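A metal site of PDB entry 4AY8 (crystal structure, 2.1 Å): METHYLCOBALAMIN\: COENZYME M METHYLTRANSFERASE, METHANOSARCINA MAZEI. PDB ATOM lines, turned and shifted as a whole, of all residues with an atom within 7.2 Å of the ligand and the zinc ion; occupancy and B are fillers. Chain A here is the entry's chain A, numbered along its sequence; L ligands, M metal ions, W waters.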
ATOM      1  N   SER A  35     -30.441  25.047   5.658  1.00  0.00           N
ATOM      2  CA  SER A  35     -29.266  24.396   5.095  1.00  0.00           C
ATOM      3  C   SER A  35     -28.174  25.422   4.891  1.00  0.00           C
ATOM      4  O   SER A  35     -28.423  26.481   4.324  1.00  0.00           O
ATOM      5  CB  SER A  35     -29.610  23.713   3.778  1.00  0.00           C
ATOM      6  OG  SER A  35     -28.481  23.059   3.246  1.00  0.00           O
ATOM      7  N   VAL A  36     -26.966  25.111   5.366  1.00  0.00           N
ATOM      8  CA  VAL A  36     -25.804  25.970   5.115  1.00  0.00           C
ATOM      9  C   VAL A  36     -24.976  25.406   3.961  1.00  0.00           C
ATOM     10  O   VAL A  36     -23.969  25.970   3.587  1.00  0.00           O
ATOM     11  CB  VAL A  36     -24.919  26.168   6.380  1.00  0.00           C
ATOM     12  CG1 VAL A  36     -25.750  26.722   7.532  1.00  0.00           C
ATOM     13  CG2 VAL A  36     -24.221  24.867   6.759  1.00  0.00           C
ATOM     14  N   THR A  37     -25.447  24.285   3.428  1.00  0.00           N
ATOM     15  CA  THR A  37     -24.834  23.635   2.283  1.00  0.00           C
ATOM     16  C   THR A  37     -25.773  23.763   1.082  1.00  0.00           C
ATOM     17  O   THR A  37     -26.891  24.268   1.210  1.00  0.00           O
ATOM     18  CB  THR A  37     -24.539  22.152   2.591  1.00  0.00           C
ATOM     19  OG1 THR A  37     -25.707  21.531   3.121  1.00  0.00           O
ATOM     20  CG2 THR A  37     -23.396  22.041   3.633  1.00  0.00           C
ATOM     21  N   GLN A  38     -25.317  23.303  -0.085  1.00  0.00           N
ATOM     22  CA  GLN A  38     -26.030  23.569  -1.333  1.00  0.00           C
ATOM     23  C   GLN A  38     -27.466  23.072  -1.284  1.00  0.00           C
ATOM     24  O   GLN A  38     -27.747  21.988  -0.751  1.00  0.00           O
ATOM     25  CB  GLN A  38     -25.256  23.011  -2.536  1.00  0.00           C
ATOM     26  CG  GLN A  38     -25.675  21.629  -3.031  1.00  0.00           C
ATOM     27  CD  GLN A  38     -26.873  21.701  -3.930  1.00  0.00           C
ATOM     28  OE1 GLN A  38     -27.125  22.725  -4.562  1.00  0.00           O
ATOM     29  NE2 GLN A  38     -27.645  20.613  -3.985  1.00  0.00           N
ATOM     30  N   THR A  39     -28.381  23.878  -1.829  1.00  0.00           N
ATOM     31  CA  THR A  39     -29.813  23.613  -1.742  1.00  0.00           C
ATOM     32  C   THR A  39     -30.530  23.423  -3.055  1.00  0.00           C
ATOM     33  O   THR A  39     -31.759  23.368  -3.083  1.00  0.00           O
ATOM     34  CB  THR A  39     -30.532  24.759  -1.029  1.00  0.00           C
ATOM     35  OG1 THR A  39     -30.269  26.002  -1.715  1.00  0.00           O
ATOM     36  CG2 THR A  39     -30.112  24.839   0.444  1.00  0.00           C
ATOM     37  N   ARG A  79     -29.665  29.888   0.534  1.00  0.00           N
ATOM     38  CA  ARG A  79     -28.264  29.557   0.391  1.00  0.00           C
ATOM     39  C   ARG A  79     -27.894  29.498  -1.100  1.00  0.00           C
ATOM     40  O   ARG A  79     -28.614  28.892  -1.894  1.00  0.00           O
ATOM     41  CB  ARG A  79     -28.003  28.202   1.033  1.00  0.00           C
ATOM     42  CG  ARG A  79     -26.569  27.926   1.458  1.00  0.00           C
ATOM     43  CD  ARG A  79     -25.694  27.486   0.309  1.00  0.00           C
ATOM     44  NE  ARG A  79     -24.424  26.867   0.731  1.00  0.00           N
ATOM     45  CZ  ARG A  79     -23.542  26.364  -0.138  1.00  0.00           C
ATOM     46  NH1 ARG A  79     -23.816  26.402  -1.424  1.00  0.00           N
ATOM     47  NH2 ARG A  79     -22.411  25.818   0.264  1.00  0.00           N
ATOM     48  N   PRO A  81     -23.997  29.846  -3.836  1.00  0.00           N
ATOM     49  CA  PRO A  81     -24.484  29.197  -5.042  1.00  0.00           C
ATOM     50  C   PRO A  81     -24.640  27.668  -4.852  1.00  0.00           C
ATOM     51  O   PRO A  81     -25.098  27.252  -3.781  1.00  0.00           O
ATOM     52  CB  PRO A  81     -23.407  29.523  -6.052  1.00  0.00           C
ATOM     53  CG  PRO A  81     -22.156  29.445  -5.228  1.00  0.00           C
ATOM     54  CD  PRO A  81     -22.528  29.976  -3.876  1.00  0.00           C
ATOM     55  N   TYR A  82     -24.263  26.865  -5.856  1.00  0.00           N
ATOM     56  CA  TYR A  82     -24.578  25.415  -5.856  1.00  0.00           C
ATOM     57  C   TYR A  82     -23.360  24.489  -5.997  1.00  0.00           C
ATOM     58  O   TYR A  82     -23.508  23.297  -6.243  1.00  0.00           O
ATOM     59  CB  TYR A  82     -25.587  25.113  -6.990  1.00  0.00           C
ATOM     60  CG  TYR A  82     -26.781  26.017  -6.899  1.00  0.00           C
ATOM     61  CD1 TYR A  82     -27.692  25.869  -5.875  1.00  0.00           C
ATOM     62  CD2 TYR A  82     -26.973  27.057  -7.802  1.00  0.00           C
ATOM     63  CE1 TYR A  82     -28.745  26.688  -5.744  1.00  0.00           C
ATOM     64  CE2 TYR A  82     -28.060  27.914  -7.669  1.00  0.00           C
ATOM     65  CZ  TYR A  82     -28.933  27.715  -6.619  1.00  0.00           C
ATOM     66  OH  TYR A  82     -30.024  28.517  -6.419  1.00  0.00           O
ATOM     67  N   CSD A  83     -22.157  25.030  -5.800  1.00  0.00           N
ATOM     68  CA  CSD A  83     -20.950  24.305  -6.141  1.00  0.00           C
ATOM     69  CB  CSD A  83     -20.744  24.499  -7.646  1.00  0.00           C
ATOM     70  SG  CSD A  83     -20.303  26.086  -7.958  1.00  0.00           S
ATOM     71  C   CSD A  83     -19.767  24.830  -5.362  1.00  0.00           C
ATOM     72  O   CSD A  83     -19.854  25.850  -4.710  1.00  0.00           O
ATOM     73  OD1 CSD A  83     -18.962  26.131  -8.423  1.00  0.00           O
ATOM     74  OD2 CSD A  83     -21.140  26.641  -8.976  1.00  0.00           O
ATOM     75  N   LEU A  84     -18.630  24.145  -5.476  1.00  0.00           N
ATOM     76  CA  LEU A  84     -17.389  24.543  -4.819  1.00  0.00           C
ATOM     77  C   LEU A  84     -16.323  25.004  -5.820  1.00  0.00           C
ATOM     78  O   LEU A  84     -15.138  24.699  -5.639  1.00  0.00           O
ATOM     79  CB  LEU A  84     -16.839  23.377  -3.984  1.00  0.00           C
ATOM     80  CG  LEU A  84     -17.724  22.996  -2.798  1.00  0.00           C
ATOM     81  CD1 LEU A  84     -17.095  21.912  -1.920  1.00  0.00           C
ATOM     82  CD2 LEU A  84     -18.065  24.245  -1.965  1.00  0.00           C
ATOM     83  N   GLN A 103     -23.143  18.356  -9.976  1.00  0.00           N
ATOM     84  CA  GLN A 103     -22.504  19.621  -9.681  1.00  0.00           C
ATOM     85  C   GLN A 103     -21.275  19.831 -10.544  1.00  0.00           C
ATOM     86  O   GLN A 103     -20.585  18.884 -10.916  1.00  0.00           O
ATOM     87  CB  GLN A 103     -22.022  19.680  -8.236  1.00  0.00           C
ATOM     88  CG  GLN A 103     -23.031  20.011  -7.151  1.00  0.00           C
ATOM     89  CD  GLN A 103     -22.340  20.060  -5.786  1.00  0.00           C
ATOM     90  OE1 GLN A 103     -21.559  19.165  -5.449  1.00  0.00           O
ATOM     91  NE2 GLN A 103     -22.568  21.124  -5.023  1.00  0.00           N
ATOM     92  N   ALA A 210     -17.183  25.516   2.867  1.00  0.00           N
ATOM     93  CA  ALA A 210     -17.113  24.067   2.807  1.00  0.00           C
ATOM     94  C   ALA A 210     -15.687  23.697   2.426  1.00  0.00           C
ATOM     95  O   ALA A 210     -15.210  24.028   1.331  1.00  0.00           O
ATOM     96  CB  ALA A 210     -18.109  23.517   1.795  1.00  0.00           C
ATOM     97  N   ASP A 211     -15.016  22.992   3.331  1.00  0.00           N
ATOM     98  CA  ASP A 211     -13.620  22.668   3.118  1.00  0.00           C
ATOM     99  C   ASP A 211     -13.372  21.158   3.226  1.00  0.00           C
ATOM    100  O   ASP A 211     -12.722  20.682   4.153  1.00  0.00           O
ATOM    101  CB  ASP A 211     -12.775  23.445   4.142  1.00  0.00           C
ATOM    102  CG  ASP A 211     -11.538  24.046   3.532  1.00  0.00           C
ATOM    103  OD1 ASP A 211     -11.158  23.599   2.425  1.00  0.00           O
ATOM    104  OD2 ASP A 211     -10.941  24.959   4.145  1.00  0.00           O
ATOM    105  N   PRO A 212     -13.888  20.386   2.249  1.00  0.00           N
ATOM    106  CA  PRO A 212     -13.800  18.922   2.350  1.00  0.00           C
ATOM    107  C   PRO A 212     -12.359  18.384   2.400  1.00  0.00           C
ATOM    108  O   PRO A 212     -12.118  17.325   2.979  1.00  0.00           O
ATOM    109  CB  PRO A 212     -14.503  18.438   1.079  1.00  0.00           C
ATOM    110  CG  PRO A 212     -14.516  19.615   0.151  1.00  0.00           C
ATOM    111  CD  PRO A 212     -14.550  20.835   1.012  1.00  0.00           C
ATOM    112  N   HIS A 246     -17.880  24.186   7.461  1.00  0.00           N
ATOM    113  CA  HIS A 246     -18.354  22.846   7.129  1.00  0.00           C
ATOM    114  C   HIS A 246     -17.192  21.952   6.705  1.00  0.00           C
ATOM    115  O   HIS A 246     -16.474  22.280   5.769  1.00  0.00           O
ATOM    116  CB  HIS A 246     -19.358  22.903   5.975  1.00  0.00           C
ATOM    117  CG  HIS A 246     -19.745  21.557   5.457  1.00  0.00           C
ATOM    118  ND1 HIS A 246     -20.615  20.728   6.118  1.00  0.00           N
ATOM    119  CD2 HIS A 246     -19.325  20.874   4.364  1.00  0.00           C
ATOM    120  CE1 HIS A 246     -20.733  19.600   5.449  1.00  0.00           C
ATOM    121  NE2 HIS A 246     -19.956  19.657   4.384  1.00  0.00           N
ATOM    122  N   ILE A 247     -17.031  20.812   7.365  1.00  0.00           N
ATOM    123  CA  ILE A 247     -16.053  19.817   6.920  1.00  0.00           C
ATOM    124  C   ILE A 247     -16.702  18.461   7.062  1.00  0.00           C
ATOM    125  O   ILE A 247     -17.109  18.064   8.154  1.00  0.00           O
ATOM    126  CB  ILE A 247     -14.724  19.865   7.741  1.00  0.00           C
ATOM    127  CG1 ILE A 247     -14.026  21.239   7.611  1.00  0.00           C
ATOM    128  CG2 ILE A 247     -13.768  18.750   7.307  1.00  0.00           C
ATOM    129  CD1 ILE A 247     -12.838  21.424   8.554  1.00  0.00           C
ATOM    130  N   CYS A 248     -16.809  17.753   5.945  1.00  0.00           N
ATOM    131  CA  CYS A 248     -17.488  16.476   5.948  1.00  0.00           C
ATOM    132  C   CYS A 248     -16.550  15.337   6.354  1.00  0.00           C
ATOM    133  O   CYS A 248     -15.372  15.549   6.630  1.00  0.00           O
ATOM    134  CB  CYS A 248     -18.218  16.219   4.599  1.00  0.00           C
ATOM    135  SG  CYS A 248     -17.577  17.064   3.124  1.00  0.00           S
ATOM    136  N   GLY A 249     -17.098  14.127   6.448  1.00  0.00           N
ATOM    137  CA  GLY A 249     -16.351  12.964   6.906  1.00  0.00           C
ATOM    138  C   GLY A 249     -16.330  12.843   8.417  1.00  0.00           C
ATOM    139  O   GLY A 249     -17.027  13.594   9.118  1.00  0.00           O
ATOM    140  N   SER A 267     -20.380  23.020  10.865  1.00  0.00           N
ATOM    141  CA  SER A 267     -21.336  22.184  10.149  1.00  0.00           C
ATOM    142  C   SER A 267     -20.704  20.818   9.916  1.00  0.00           C
ATOM    143  O   SER A 267     -19.656  20.723   9.285  1.00  0.00           O
ATOM    144  CB  SER A 267     -21.734  22.807   8.819  1.00  0.00           C
ATOM    145  OG  SER A 267     -22.434  21.881   7.981  1.00  0.00           O
ATOM    146  N   GLU A 269     -21.352  16.266   9.397  1.00  0.00           N
ATOM    147  CA  GLU A 269     -22.197  15.181   8.935  1.00  0.00           C
ATOM    148  C   GLU A 269     -22.561  14.247  10.086  1.00  0.00           C
ATOM    149  O   GLU A 269     -22.132  14.430  11.228  1.00  0.00           O
ATOM    150  CB  GLU A 269     -21.452  14.341   7.881  1.00  0.00           C
ATOM    151  CG  GLU A 269     -21.144  15.022   6.588  1.00  0.00           C
ATOM    152  CD  GLU A 269     -20.742  14.023   5.513  1.00  0.00           C
ATOM    153  OE1 GLU A 269     -19.644  13.412   5.635  1.00  0.00           O
ATOM    154  OE2 GLU A 269     -21.550  13.837   4.573  1.00  0.00           O
ATOM    155  N   GLY A 324     -26.388  17.166   6.739  1.00  0.00           N
ATOM    156  CA  GLY A 324     -24.979  16.937   7.032  1.00  0.00           C
ATOM    157  C   GLY A 324     -24.011  17.443   5.987  1.00  0.00           C
ATOM    158  O   GLY A 324     -22.895  17.840   6.321  1.00  0.00           O
ATOM    159  N   CYS A 325     -24.418  17.417   4.724  1.00  0.00           N
ATOM    160  CA  CYS A 325     -23.597  17.909   3.609  1.00  0.00           C
ATOM    161  C   CYS A 325     -24.543  18.579   2.609  1.00  0.00           C
ATOM    162  O   CYS A 325     -25.690  18.910   2.961  1.00  0.00           O
ATOM    163  CB  CYS A 325     -22.824  16.737   2.962  1.00  0.00           C
ATOM    164  SG  CYS A 325     -21.453  17.190   1.847  1.00  0.00           S
ATOM    165  N   GLY A 326     -24.076  18.808   1.390  1.00  0.00           N
ATOM    166  CA  GLY A 326     -24.930  19.299   0.316  1.00  0.00           C
ATOM    167  C   GLY A 326     -26.167  18.423   0.168  1.00  0.00           C
ATOM    168  O   GLY A 326     -26.092  17.216   0.303  1.00  0.00           O
ATOM    169  N   ILE A 327     -27.318  19.044  -0.085  1.00  0.00           N
ATOM    170  CA  ILE A 327     -28.513  18.273  -0.395  1.00  0.00           C
ATOM    171  C   ILE A 327     -28.305  17.603  -1.746  1.00  0.00           C
ATOM    172  O   ILE A 327     -27.886  18.256  -2.707  1.00  0.00           O
ATOM    173  CB  ILE A 327     -29.773  19.148  -0.416  1.00  0.00           C
ATOM    174  CG1 ILE A 327     -29.928  19.878   0.931  1.00  0.00           C
ATOM    175  CG2 ILE A 327     -31.032  18.289  -0.742  1.00  0.00           C
ATOM    176  CD1 ILE A 327     -31.161  20.780   1.032  1.00  0.00           C
ATOM    177  N   ALA A 328     -28.521  16.300  -1.804  1.00  0.00           N
ATOM    178  CA  ALA A 328     -28.419  15.577  -3.075  1.00  0.00           C
ATOM    179  C   ALA A 328     -29.506  16.099  -4.018  1.00  0.00           C
ATOM    180  O   ALA A 328     -30.659  16.244  -3.625  1.00  0.00           O
ATOM    181  CB  ALA A 328     -28.554  14.062  -2.857  1.00  0.00           C
HETATM  182  C1  LIG L   1     -20.306  20.247   0.472  1.00  0.00           C
HETATM  183  C2  LIG L   1     -20.323  21.010  -0.837  1.00  0.00           C
HETATM  184  S1  LIG L   1     -18.638  19.670   0.941  1.00  0.00           S
HETATM  185  S2  LIG L   1     -21.853  21.486  -1.340  1.00  0.00           S
HETATM  186  O1  LIG L   1     -22.619  20.323  -1.799  1.00  0.00           O
HETATM  187  O2  LIG L   1     -21.650  22.376  -2.510  1.00  0.00           O
HETATM  188  O3  LIG L   1     -22.621  22.189  -0.307  1.00  0.00           O
HETATM  189 ZN    ZN M   1     -19.555  18.364   2.683  1.00  0.00          ZN
HETATM  190  O   HOH W   1     -21.539  25.112  -2.355  1.00  0.00           O
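The backbone NH (N) of Gln 38 sits at hydrogen-bond distance from an oxygen (O3) of the ligand.
The guanidinium group of Arg 79 is in salt-bridge range of an oxygen (O3) of the ligand, 3.7 Å away.
The side-chain amide nitrogen (NE2) of Gln 103 is in hydrogen-bond range of an oxygen (O2) of the ligand, 3.0 Å away.
The backbone carbonyl oxygen of Thr 37 is in hydrogen-bond range of the side-chain hydroxyl of Ser 35.
The backbone carbonyl oxygen (O) of His 246 sits at hydrogen-bond distance from the backbone NH (N) of Asp 211, 2.9 Å away.
The guanidinium group (NH1) of Arg 79 lies within hydrogen-bond range of the backbone carbonyl oxygen (O) of Pro 81 (2.8 Å).
NE2 of Gln 38 lies within hydrogen-bond range of O of Ile 327, at 2.7 Å.
O of Val 36 lies within hydrogen-bond range of NE of Arg 79, 3.0 Å away.
The backbone carbonyl oxygen (O) of Arg 79 lies within hydrogen-bond range of the side-chain hydroxyl (OG1) of Thr 39, 3.3 Å away.
A ring nitrogen (ND1) of His 246 sits at hydrogen-bond distance from the side-chain hydroxyl (OG) of Ser 267 (2.8 Å).
O of Cys 325 lies within hydrogen-bond range of OG1 of Thr 37 (2.6 Å).
Water W1 lies within hydrogen-bond range of O2 of the ligand (2.7 Å), NH1 of Arg 79 (2.8 Å) and O of CSD 83 (3.0 Å).
The zinc ion is bound by a ring nitrogen (NE2) of His 246 (2.2 Å), a sulfur (S1) of the ligand (2.4 Å), the side-chain sulfur of Cys 325 (2.4 Å) and the side-chain sulfur of Cys 248 (2.4 Å).
Merely in contact with the ligand: Gly 326 (3.3 Å), Thr 37 (3.5 Å), Leu 84 (3.5 Å) and Ala 210 (3.98 Å).
Of the 25 residues printed, 10 come within 4 Å of the ligand.
Along chain A the residues within 4 Å of the ligand span positions 37 to 326.
The nearest printed residue that does not touch the ligand is CSD 83 (4.2 Å).
Of the 25 residues printed, 3 come within 4 Å of the zinc ion.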
